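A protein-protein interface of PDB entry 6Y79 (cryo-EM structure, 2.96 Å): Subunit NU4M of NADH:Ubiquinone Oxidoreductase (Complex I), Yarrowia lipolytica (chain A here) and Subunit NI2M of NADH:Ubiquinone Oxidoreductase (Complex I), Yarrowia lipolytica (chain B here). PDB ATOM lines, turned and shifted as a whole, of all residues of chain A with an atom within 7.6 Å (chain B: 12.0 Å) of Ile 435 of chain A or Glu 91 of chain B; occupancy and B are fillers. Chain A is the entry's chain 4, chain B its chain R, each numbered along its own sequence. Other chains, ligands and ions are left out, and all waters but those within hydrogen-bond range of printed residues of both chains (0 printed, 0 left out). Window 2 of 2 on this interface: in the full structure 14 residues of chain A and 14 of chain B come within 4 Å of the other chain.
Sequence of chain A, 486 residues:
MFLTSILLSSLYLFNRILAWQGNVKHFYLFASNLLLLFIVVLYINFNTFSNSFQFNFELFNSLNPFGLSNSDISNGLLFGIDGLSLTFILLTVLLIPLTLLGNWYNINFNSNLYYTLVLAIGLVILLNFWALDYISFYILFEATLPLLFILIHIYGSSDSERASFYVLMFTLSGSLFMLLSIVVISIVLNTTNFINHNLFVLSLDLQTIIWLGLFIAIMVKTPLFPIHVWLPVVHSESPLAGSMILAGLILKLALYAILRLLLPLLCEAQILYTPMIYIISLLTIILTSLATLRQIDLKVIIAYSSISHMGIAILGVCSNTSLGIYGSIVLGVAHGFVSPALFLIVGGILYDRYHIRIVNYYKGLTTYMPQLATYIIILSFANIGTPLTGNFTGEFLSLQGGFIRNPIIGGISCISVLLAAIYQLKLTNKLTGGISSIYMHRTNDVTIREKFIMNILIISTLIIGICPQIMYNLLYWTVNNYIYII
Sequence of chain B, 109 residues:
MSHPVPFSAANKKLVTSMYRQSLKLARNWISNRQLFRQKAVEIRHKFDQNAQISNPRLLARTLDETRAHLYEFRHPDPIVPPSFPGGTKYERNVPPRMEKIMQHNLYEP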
ATOM      1  N   TYR A 362     -20.056 -20.280 -18.560  1.00  0.00           N
ATOM      2  CA  TYR A 362     -19.280 -21.060 -17.608  1.00  0.00           C
ATOM      3  C   TYR A 362     -18.901 -22.391 -18.242  1.00  0.00           C
ATOM      4  O   TYR A 362     -19.773 -23.178 -18.616  1.00  0.00           O
ATOM      5  CB  TYR A 362     -20.086 -21.266 -16.334  1.00  0.00           C
ATOM      6  CG  TYR A 362     -20.339 -20.014 -15.546  1.00  0.00           C
ATOM      7  CD1 TYR A 362     -19.333 -19.105 -15.309  1.00  0.00           C
ATOM      8  CD2 TYR A 362     -21.597 -19.723 -15.075  1.00  0.00           C
ATOM      9  CE1 TYR A 362     -19.566 -17.953 -14.593  1.00  0.00           C
ATOM     10  CE2 TYR A 362     -21.843 -18.580 -14.359  1.00  0.00           C
ATOM     11  CZ  TYR A 362     -20.825 -17.700 -14.122  1.00  0.00           C
ATOM     12  OH  TYR A 362     -21.066 -16.556 -13.414  1.00  0.00           O
ATOM     13  N   LYS A 363     -17.602 -22.639 -18.358  1.00  0.00           N
ATOM     14  CA  LYS A 363     -17.091 -23.866 -18.947  1.00  0.00           C
ATOM     15  C   LYS A 363     -15.668 -24.070 -18.459  1.00  0.00           C
ATOM     16  O   LYS A 363     -14.885 -23.121 -18.419  1.00  0.00           O
ATOM     17  CB  LYS A 363     -17.123 -23.807 -20.475  1.00  0.00           C
ATOM     18  CG  LYS A 363     -16.717 -25.094 -21.152  1.00  0.00           C
ATOM     19  CD  LYS A 363     -16.836 -25.002 -22.654  1.00  0.00           C
ATOM     20  CE  LYS A 363     -15.816 -24.050 -23.208  1.00  0.00           C
ATOM     21  NZ  LYS A 363     -15.672 -24.203 -24.669  1.00  0.00           N
ATOM     22  N   GLY A 364     -15.347 -25.303 -18.082  1.00  0.00           N
ATOM     23  CA  GLY A 364     -13.985 -25.668 -17.756  1.00  0.00           C
ATOM     24  C   GLY A 364     -13.448 -25.021 -16.506  1.00  0.00           C
ATOM     25  O   GLY A 364     -12.342 -24.480 -16.505  1.00  0.00           O
ATOM     26  N   LEU A 365     -14.222 -25.070 -15.431  1.00  0.00           N
ATOM     27  CA  LEU A 365     -13.835 -24.424 -14.186  1.00  0.00           C
ATOM     28  C   LEU A 365     -12.794 -25.206 -13.387  1.00  0.00           C
ATOM     29  O   LEU A 365     -12.337 -24.689 -12.368  1.00  0.00           O
ATOM     30  CB  LEU A 365     -15.080 -24.183 -13.321  1.00  0.00           C
ATOM     31  CG  LEU A 365     -15.907 -22.899 -13.442  1.00  0.00           C
ATOM     32  CD1 LEU A 365     -16.734 -22.874 -14.710  1.00  0.00           C
ATOM     33  CD2 LEU A 365     -16.811 -22.786 -12.244  1.00  0.00           C
ATOM     34  N   THR A 367      -9.666 -26.130 -14.286  1.00  0.00           N
ATOM     35  CA  THR A 367      -8.256 -25.907 -14.551  1.00  0.00           C
ATOM     36  C   THR A 367      -7.733 -24.655 -13.871  1.00  0.00           C
ATOM     37  O   THR A 367      -6.523 -24.531 -13.682  1.00  0.00           O
ATOM     38  CB  THR A 367      -8.012 -25.857 -16.057  1.00  0.00           C
ATOM     39  OG1 THR A 367      -6.616 -25.666 -16.306  1.00  0.00           O
ATOM     40  CG2 THR A 367      -8.796 -24.740 -16.688  1.00  0.00           C
ATOM     41  N   LYS A 430     -20.917 -29.760 -17.535  1.00  0.00           N
ATOM     42  CA  LYS A 430     -20.725 -28.515 -18.267  1.00  0.00           C
ATOM     43  C   LYS A 430     -19.877 -27.536 -17.469  1.00  0.00           C
ATOM     44  O   LYS A 430     -19.000 -26.870 -18.027  1.00  0.00           O
ATOM     45  CB  LYS A 430     -22.081 -27.898 -18.602  1.00  0.00           C
ATOM     46  CG  LYS A 430     -22.018 -26.524 -19.225  1.00  0.00           C
ATOM     47  CD  LYS A 430     -21.420 -26.583 -20.608  1.00  0.00           C
ATOM     48  CE  LYS A 430     -21.500 -25.243 -21.318  1.00  0.00           C
ATOM     49  NZ  LYS A 430     -22.881 -24.931 -21.784  1.00  0.00           N
ATOM     50  N   LEU A 431     -20.118 -27.442 -16.160  1.00  0.00           N
ATOM     51  CA  LEU A 431     -19.343 -26.517 -15.340  1.00  0.00           C
ATOM     52  C   LEU A 431     -17.911 -26.990 -15.159  1.00  0.00           C
ATOM     53  O   LEU A 431     -16.980 -26.182 -15.197  1.00  0.00           O
ATOM     54  CB  LEU A 431     -19.995 -26.333 -13.973  1.00  0.00           C
ATOM     55  CG  LEU A 431     -21.312 -25.573 -13.887  1.00  0.00           C
ATOM     56  CD1 LEU A 431     -21.787 -25.570 -12.459  1.00  0.00           C
ATOM     57  CD2 LEU A 431     -21.141 -24.176 -14.381  1.00  0.00           C
ATOM     58  N   THR A 432     -17.708 -28.287 -14.954  1.00  0.00           N
ATOM     59  CA  THR A 432     -16.360 -28.742 -14.664  1.00  0.00           C
ATOM     60  C   THR A 432     -15.577 -29.020 -15.945  1.00  0.00           C
ATOM     61  O   THR A 432     -14.422 -28.617 -16.053  1.00  0.00           O
ATOM     62  CB  THR A 432     -16.417 -29.960 -13.739  1.00  0.00           C
ATOM     63  OG1 THR A 432     -17.206 -30.999 -14.328  1.00  0.00           O
ATOM     64  CG2 THR A 432     -17.068 -29.561 -12.421  1.00  0.00           C
ATOM     65  N   GLY A 433     -16.202 -29.596 -16.969  1.00  0.00           N
ATOM     66  CA  GLY A 433     -15.501 -30.037 -18.153  1.00  0.00           C
ATOM     67  C   GLY A 433     -15.290 -28.958 -19.205  1.00  0.00           C
ATOM     68  O   GLY A 433     -15.926 -27.910 -19.209  1.00  0.00           O
ATOM     69  N   GLY A 434     -14.363 -29.251 -20.113  1.00  0.00           N
ATOM     70  CA  GLY A 434     -14.052 -28.397 -21.242  1.00  0.00           C
ATOM     71  C   GLY A 434     -12.777 -27.589 -21.044  1.00  0.00           C
ATOM     72  O   GLY A 434     -12.169 -27.558 -19.972  1.00  0.00           O
ATOM     73  N   ILE A 435     -12.352 -26.941 -22.133  1.00  0.00           N
ATOM     74  CA  ILE A 435     -11.333 -25.904 -22.030  1.00  0.00           C
ATOM     75  C   ILE A 435     -11.946 -24.745 -21.261  1.00  0.00           C
ATOM     76  O   ILE A 435     -13.163 -24.533 -21.310  1.00  0.00           O
ATOM     77  CB  ILE A 435     -10.840 -25.496 -23.433  1.00  0.00           C
ATOM     78  CG1 ILE A 435     -10.270 -26.710 -24.163  1.00  0.00           C
ATOM     79  CG2 ILE A 435      -9.772 -24.424 -23.408  1.00  0.00           C
ATOM     80  CD1 ILE A 435     -10.017 -26.472 -25.627  1.00  0.00           C
ATOM     81  N   SER A 436     -11.115 -24.053 -20.477  1.00  0.00           N
ATOM     82  CA  SER A 436     -11.524 -22.869 -19.731  1.00  0.00           C
ATOM     83  C   SER A 436     -12.203 -21.837 -20.622  1.00  0.00           C
ATOM     84  O   SER A 436     -11.896 -21.712 -21.810  1.00  0.00           O
ATOM     85  CB  SER A 436     -10.310 -22.242 -19.060  1.00  0.00           C
ATOM     86  OG  SER A 436     -10.672 -21.056 -18.386  1.00  0.00           O
ATOM     87  N   SER A 437     -13.152 -21.119 -20.037  1.00  0.00           N
ATOM     88  CA  SER A 437     -14.022 -20.242 -20.802  1.00  0.00           C
ATOM     89  C   SER A 437     -13.268 -19.017 -21.292  1.00  0.00           C
ATOM     90  O   SER A 437     -12.433 -18.453 -20.583  1.00  0.00           O
ATOM     91  CB  SER A 437     -15.207 -19.816 -19.947  1.00  0.00           C
ATOM     92  OG  SER A 437     -16.083 -18.966 -20.659  1.00  0.00           O
ATOM     93  N   ILE A 438     -13.559 -18.616 -22.529  1.00  0.00           N
ATOM     94  CA  ILE A 438     -12.944 -17.422 -23.080  1.00  0.00           C
ATOM     95  C   ILE A 438     -13.636 -16.171 -22.575  1.00  0.00           C
ATOM     96  O   ILE A 438     -13.090 -15.071 -22.697  1.00  0.00           O
ATOM     97  CB  ILE A 438     -12.953 -17.484 -24.613  1.00  0.00           C
ATOM     98  CG1 ILE A 438     -14.379 -17.591 -25.127  1.00  0.00           C
ATOM     99  CG2 ILE A 438     -12.141 -18.665 -25.090  1.00  0.00           C
ATOM    100  CD1 ILE A 438     -14.466 -17.563 -26.607  1.00  0.00           C
ATOM    101  N   VAL B  80      -8.691 -40.574 -39.140  1.00  0.00           N
ATOM    102  CA  VAL B  80      -8.234 -39.268 -38.656  1.00  0.00           C
ATOM    103  C   VAL B  80      -6.948 -39.513 -37.875  1.00  0.00           C
ATOM    104  O   VAL B  80      -6.827 -40.557 -37.219  1.00  0.00           O
ATOM    105  CB  VAL B  80      -9.287 -38.587 -37.757  1.00  0.00           C
ATOM    106  CG1 VAL B  80      -9.006 -37.108 -37.546  1.00  0.00           C
ATOM    107  CG2 VAL B  80     -10.687 -38.759 -38.311  1.00  0.00           C
ATOM    108  N   PRO B  81      -5.960 -38.621 -37.903  1.00  0.00           N
ATOM    109  CA  PRO B  81      -4.881 -38.732 -36.941  1.00  0.00           C
ATOM    110  C   PRO B  81      -5.364 -38.218 -35.601  1.00  0.00           C
ATOM    111  O   PRO B  81      -6.174 -37.279 -35.548  1.00  0.00           O
ATOM    112  CB  PRO B  81      -3.773 -37.840 -37.526  1.00  0.00           C
ATOM    113  CG  PRO B  81      -4.237 -37.463 -38.872  1.00  0.00           C
ATOM    114  CD  PRO B  81      -5.697 -37.502 -38.814  1.00  0.00           C
ATOM    115  N   PRO B  82      -4.897 -38.815 -34.509  1.00  0.00           N
ATOM    116  CA  PRO B  82      -5.602 -38.669 -33.229  1.00  0.00           C
ATOM    117  C   PRO B  82      -5.548 -37.280 -32.625  1.00  0.00           C
ATOM    118  O   PRO B  82      -6.511 -36.876 -31.965  1.00  0.00           O
ATOM    119  CB  PRO B  82      -4.894 -39.694 -32.338  1.00  0.00           C
ATOM    120  CG  PRO B  82      -3.593 -39.855 -32.972  1.00  0.00           C
ATOM    121  CD  PRO B  82      -3.814 -39.795 -34.415  1.00  0.00           C
ATOM    122  N   SER B  83      -4.494 -36.512 -32.865  1.00  0.00           N
ATOM    123  CA  SER B  83      -4.369 -35.189 -32.267  1.00  0.00           C
ATOM    124  C   SER B  83      -5.145 -34.115 -33.018  1.00  0.00           C
ATOM    125  O   SER B  83      -4.965 -32.930 -32.731  1.00  0.00           O
ATOM    126  CB  SER B  83      -2.896 -34.794 -32.177  1.00  0.00           C
ATOM    127  OG  SER B  83      -2.347 -34.610 -33.467  1.00  0.00           O
ATOM    128  N   PHE B  84      -6.000 -34.502 -33.952  1.00  0.00           N
ATOM    129  CA  PHE B  84      -6.757 -33.640 -34.841  1.00  0.00           C
ATOM    130  C   PHE B  84      -8.247 -33.842 -34.583  1.00  0.00           C
ATOM    131  O   PHE B  84      -8.636 -34.886 -34.047  1.00  0.00           O
ATOM    132  CB  PHE B  84      -6.363 -33.977 -36.287  1.00  0.00           C
ATOM    133  CG  PHE B  84      -5.005 -33.481 -36.653  1.00  0.00           C
ATOM    134  CD1 PHE B  84      -4.407 -32.449 -35.940  1.00  0.00           C
ATOM    135  CD2 PHE B  84      -4.316 -34.045 -37.689  1.00  0.00           C
ATOM    136  CE1 PHE B  84      -3.149 -32.002 -36.267  1.00  0.00           C
ATOM    137  CE2 PHE B  84      -3.075 -33.598 -38.007  1.00  0.00           C
ATOM    138  CZ  PHE B  84      -2.486 -32.579 -37.305  1.00  0.00           C
ATOM    139  N   PRO B  85      -9.110 -32.868 -34.938  1.00  0.00           N
ATOM    140  CA  PRO B  85     -10.454 -32.782 -34.322  1.00  0.00           C
ATOM    141  C   PRO B  85     -11.394 -33.969 -34.496  1.00  0.00           C
ATOM    142  O   PRO B  85     -12.416 -34.013 -33.800  1.00  0.00           O
ATOM    143  CB  PRO B  85     -11.052 -31.536 -34.987  1.00  0.00           C
ATOM    144  CG  PRO B  85     -10.231 -31.322 -36.180  1.00  0.00           C
ATOM    145  CD  PRO B  85      -8.876 -31.636 -35.706  1.00  0.00           C
ATOM    146  N   GLY B  86     -11.102 -34.926 -35.360  1.00  0.00           N
ATOM    147  CA  GLY B  86     -11.878 -36.144 -35.294  1.00  0.00           C
ATOM    148  C   GLY B  86     -11.314 -37.203 -34.382  1.00  0.00           C
ATOM    149  O   GLY B  86     -12.010 -38.163 -34.055  1.00  0.00           O
ATOM    150  N   GLY B  87     -10.073 -37.033 -33.931  1.00  0.00           N
ATOM    151  CA  GLY B  87      -9.310 -38.125 -33.372  1.00  0.00           C
ATOM    152  C   GLY B  87      -9.405 -38.251 -31.866  1.00  0.00           C
ATOM    153  O   GLY B  87     -10.140 -37.541 -31.186  1.00  0.00           O
ATOM    154  N   THR B  88      -8.605 -39.179 -31.347  1.00  0.00           N
ATOM    155  CA  THR B  88      -8.670 -39.625 -29.966  1.00  0.00           C
ATOM    156  C   THR B  88      -7.729 -38.875 -29.037  1.00  0.00           C
ATOM    157  O   THR B  88      -7.973 -38.852 -27.829  1.00  0.00           O
ATOM    158  CB  THR B  88      -8.346 -41.116 -29.896  1.00  0.00           C
ATOM    159  OG1 THR B  88      -6.945 -41.304 -30.121  1.00  0.00           O
ATOM    160  CG2 THR B  88      -9.107 -41.858 -30.963  1.00  0.00           C
ATOM    161  N   LYS B  89      -6.655 -38.290 -29.556  1.00  0.00           N
ATOM    162  CA  LYS B  89      -5.727 -37.490 -28.773  1.00  0.00           C
ATOM    163  C   LYS B  89      -6.097 -36.018 -28.795  1.00  0.00           C
ATOM    164  O   LYS B  89      -5.333 -35.187 -28.303  1.00  0.00           O
ATOM    165  CB  LYS B  89      -4.303 -37.674 -29.305  1.00  0.00           C
ATOM    166  CG  LYS B  89      -3.183 -37.625 -28.282  1.00  0.00           C
ATOM    167  CD  LYS B  89      -1.891 -37.185 -28.956  1.00  0.00           C
ATOM    168  CE  LYS B  89      -0.861 -36.746 -27.948  1.00  0.00           C
ATOM    169  NZ  LYS B  89      -0.451 -37.907 -27.126  1.00  0.00           N
ATOM    170  N   TYR B  90      -7.246 -35.679 -29.363  1.00  0.00           N
ATOM    171  CA  TYR B  90      -7.622 -34.287 -29.545  1.00  0.00           C
ATOM    172  C   TYR B  90      -8.080 -33.703 -28.221  1.00  0.00           C
ATOM    173  O   TYR B  90      -9.000 -34.236 -27.596  1.00  0.00           O
ATOM    174  CB  TYR B  90      -8.723 -34.181 -30.591  1.00  0.00           C
ATOM    175  CG  TYR B  90      -9.168 -32.775 -30.901  1.00  0.00           C
ATOM    176  CD1 TYR B  90      -8.297 -31.860 -31.471  1.00  0.00           C
ATOM    177  CD2 TYR B  90     -10.468 -32.372 -30.651  1.00  0.00           C
ATOM    178  CE1 TYR B  90      -8.705 -30.578 -31.765  1.00  0.00           C
ATOM    179  CE2 TYR B  90     -10.882 -31.093 -30.942  1.00  0.00           C
ATOM    180  CZ  TYR B  90      -9.997 -30.202 -31.499  1.00  0.00           C
ATOM    181  OH  TYR B  90     -10.410 -28.925 -31.788  1.00  0.00           O
ATOM    182  N   GLU B  91      -7.411 -32.624 -27.797  1.00  0.00           N
ATOM    183  CA  GLU B  91      -7.688 -31.891 -26.555  1.00  0.00           C
ATOM    184  C   GLU B  91      -7.556 -32.777 -25.321  1.00  0.00           C
ATOM    185  O   GLU B  91      -8.444 -32.825 -24.473  1.00  0.00           O
ATOM    186  CB  GLU B  91      -9.062 -31.224 -26.589  1.00  0.00           C
ATOM    187  CG  GLU B  91      -9.226 -30.199 -27.664  1.00  0.00           C
ATOM    188  CD  GLU B  91     -10.634 -29.658 -27.721  1.00  0.00           C
ATOM    189  OE1 GLU B  91     -11.518 -30.224 -27.044  1.00  0.00           O
ATOM    190  OE2 GLU B  91     -10.860 -28.665 -28.443  1.00  0.00           O
ATOM    191  N   ARG B  92      -6.432 -33.476 -25.209  1.00  0.00           N
ATOM    192  CA  ARG B  92      -6.199 -34.219 -23.979  1.00  0.00           C
ATOM    193  C   ARG B  92      -5.680 -33.302 -22.879  1.00  0.00           C
ATOM    194  O   ARG B  92      -6.332 -33.125 -21.846  1.00  0.00           O
ATOM    195  CB  ARG B  92      -5.246 -35.382 -24.229  1.00  0.00           C
ATOM    196  CG  ARG B  92      -5.974 -36.614 -24.680  1.00  0.00           C
ATOM    197  CD  ARG B  92      -5.023 -37.712 -25.046  1.00  0.00           C
ATOM    198  NE  ARG B  92      -4.490 -38.391 -23.878  1.00  0.00           N
ATOM    199  CZ  ARG B  92      -3.514 -39.285 -23.931  1.00  0.00           C
ATOM    200  NH1 ARG B  92      -2.968 -39.588 -25.091  1.00  0.00           N
ATOM    201  NH2 ARG B  92      -3.072 -39.872 -22.832  1.00  0.00           N
ATOM    202  N   ASN B  93      -4.524 -32.687 -23.091  1.00  0.00           N
ATOM    203  CA  ASN B  93      -3.990 -31.724 -22.136  1.00  0.00           C
ATOM    204  C   ASN B  93      -3.781 -30.408 -22.866  1.00  0.00           C
ATOM    205  O   ASN B  93      -2.681 -30.097 -23.327  1.00  0.00           O
ATOM    206  CB  ASN B  93      -2.745 -32.235 -21.522  1.00  0.00           C
ATOM    207  CG  ASN B  93      -3.012 -33.330 -20.518  1.00  0.00           C
ATOM    208  OD1 ASN B  93      -2.414 -34.399 -20.573  1.00  0.00           O
ATOM    209  ND2 ASN B  93      -3.926 -33.068 -19.592  1.00  0.00           N
ATOM    210  N   VAL B  94      -4.857 -29.641 -22.974  1.00  0.00           N
ATOM    211  CA  VAL B  94      -4.809 -28.279 -23.483  1.00  0.00           C
ATOM    212  C   VAL B  94      -4.036 -27.465 -22.458  1.00  0.00           C
ATOM    213  O   VAL B  94      -4.422 -27.454 -21.281  1.00  0.00           O
ATOM    214  CB  VAL B  94      -6.220 -27.720 -23.706  1.00  0.00           C
ATOM    215  CG1 VAL B  94      -6.166 -26.231 -23.990  1.00  0.00           C
ATOM    216  CG2 VAL B  94      -6.905 -28.471 -24.827  1.00  0.00           C
ATOM    217  N   PRO B  95      -2.932 -26.823 -22.829  1.00  0.00           N
ATOM    218  CA  PRO B  95      -2.203 -26.003 -21.873  1.00  0.00           C
ATOM    219  C   PRO B  95      -3.009 -24.774 -21.506  1.00  0.00           C
ATOM    220  O   PRO B  95      -3.555 -24.098 -22.390  1.00  0.00           O
ATOM    221  CB  PRO B  95      -0.923 -25.629 -22.633  1.00  0.00           C
ATOM    222  CG  PRO B  95      -0.816 -26.627 -23.719  1.00  0.00           C
ATOM    223  CD  PRO B  95      -2.221 -26.918 -24.111  1.00  0.00           C
ATOM    224  N   PRO B  96      -3.147 -24.482 -20.216  1.00  0.00           N
ATOM    225  CA  PRO B  96      -3.900 -23.294 -19.812  1.00  0.00           C
ATOM    226  C   PRO B  96      -3.152 -22.029 -20.190  1.00  0.00           C
ATOM    227  O   PRO B  96      -1.920 -21.987 -20.159  1.00  0.00           O
ATOM    228  CB  PRO B  96      -4.011 -23.447 -18.293  1.00  0.00           C
ATOM    229  CG  PRO B  96      -2.863 -24.301 -17.923  1.00  0.00           C
ATOM    230  CD  PRO B  96      -2.642 -25.237 -19.059  1.00  0.00           C
ATOM    231  N   ARG B  97      -3.901 -21.006 -20.582  1.00  0.00           N
ATOM    232  CA  ARG B  97      -3.268 -19.755 -20.956  1.00  0.00           C
ATOM    233  C   ARG B  97      -2.751 -19.048 -19.708  1.00  0.00           C
ATOM    234  O   ARG B  97      -3.298 -19.204 -18.614  1.00  0.00           O
ATOM    235  CB  ARG B  97      -4.243 -18.874 -21.735  1.00  0.00           C
ATOM    236  CG  ARG B  97      -5.380 -18.304 -20.931  1.00  0.00           C
ATOM    237  CD  ARG B  97      -6.398 -17.638 -21.829  1.00  0.00           C
ATOM    238  NE  ARG B  97      -7.054 -18.599 -22.708  1.00  0.00           N
ATOM    239  CZ  ARG B  97      -8.115 -19.322 -22.366  1.00  0.00           C
ATOM    240  NH1 ARG B  97      -8.647 -19.208 -21.160  1.00  0.00           N
ATOM    241  NH2 ARG B  97      -8.646 -20.166 -23.237  1.00  0.00           N
ATOM    242  N   MET B  98      -1.654 -18.315 -19.865  1.00  0.00           N
ATOM    243  CA  MET B  98      -1.020 -17.668 -18.723  1.00  0.00           C
ATOM    244  C   MET B  98      -1.828 -16.446 -18.326  1.00  0.00           C
ATOM    245  O   MET B  98      -1.891 -15.462 -19.069  1.00  0.00           O
ATOM    246  CB  MET B  98       0.421 -17.295 -19.052  1.00  0.00           C
ATOM    247  CG  MET B  98       1.332 -18.497 -19.125  1.00  0.00           C
ATOM    248  SD  MET B  98       1.029 -19.604 -17.740  1.00  0.00           S
ATOM    249  CE  MET B  98       1.942 -21.033 -18.279  1.00  0.00           C
ATOM    250  N   GLU B  99      -2.453 -16.508 -17.157  1.00  0.00           N
ATOM    251  CA  GLU B  99      -3.338 -15.456 -16.689  1.00  0.00           C
ATOM    252  C   GLU B  99      -3.055 -15.174 -15.229  1.00  0.00           C
ATOM    253  O   GLU B  99      -3.003 -16.099 -14.416  1.00  0.00           O
ATOM    254  CB  GLU B  99      -4.801 -15.849 -16.863  1.00  0.00           C
ATOM    255  CG  GLU B  99      -5.335 -15.652 -18.255  1.00  0.00           C
ATOM    256  CD  GLU B  99      -6.785 -16.051 -18.361  1.00  0.00           C
ATOM    257  OE1 GLU B  99      -7.258 -16.772 -17.464  1.00  0.00           O
ATOM    258  OE2 GLU B  99      -7.455 -15.645 -19.330  1.00  0.00           O
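No residue of chain B comes within 4 Å of Lys 363 of chain A. No residue of chain B comes within 4 Å of Gly 364 of chain A. Of the printed residues of chain B, Thr 367 of chain A touches Pro 96. No residue of chain B comes within 4 Å of Gly 434 of chain A. Ile 435 of chain A touches just these residues of chain B: Glu 91 and Val 94. Of chain B, only Arg 97 (3.9 Å) comes within 4 Å of Ser 437 of chain A. Glu 91 of chain B touches just one residue of chain A: Ile 435. Printed residues of chain A within 4 Å of Val 94 of chain B: Ile 435 (3.8 Å). Of the printed residues of chain A, Pro 96 of chain B touches Thr 367. Of the printed residues of chain A, Arg 97 of chain B touches Ser 436 and Ser 437. The nearest residue of chain B that does not touch Ile 435 of chain A is Arg 97 of chain B (4.4 Å). The nearest residue of chain A that does not touch Glu 91 of chain B is Gly 434 of chain A (6.6 Å). The nearest printed residue of chain A that does not touch Val 94 of chain B is Thr 367 of chain A (5.7 Å).
The backbone carbonyl oxygen of Lys 363 of chain A sits at hydrogen-bond distance from the backbone NH of Ser 437 of chain A (3.1 Å). The side-chain hydroxyl (OH) of Tyr 90 of chain B lies within hydrogen-bond range of the side-chain carboxylate (OE2) of Glu 91 of chain B (3.4 Å).
OG1 of Thr 367 of chain A touches CB of Pro 96 of chain B, at 3.96 Å. OE2 of Glu 91 of chain B touches CD1 of Ile 435 of chain A (3.7 Å). CG2 of Val 94 of chain B touches CD1 of Ile 435 of chain A, 3.8 Å away. Arg 97 of chain B touches Ser 436 of chain A (NH2 to O, 3.9 Å). Ser 437 of chain A touches Arg 97 of chain B (O to NH1, 3.9 Å).
Of the 20 printed residues of chain B, 4 touch a printed residue of chain A. Printed residues of chain B that touch a printed residue of chain A: Glu 91, Val 94, Pro 96 and Arg 97. Of the 14 printed residues of chain A, 4 touch a printed residue of chain B. Along chain A the printed residues that touch a printed residue of chain B span positions 367 to 437.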
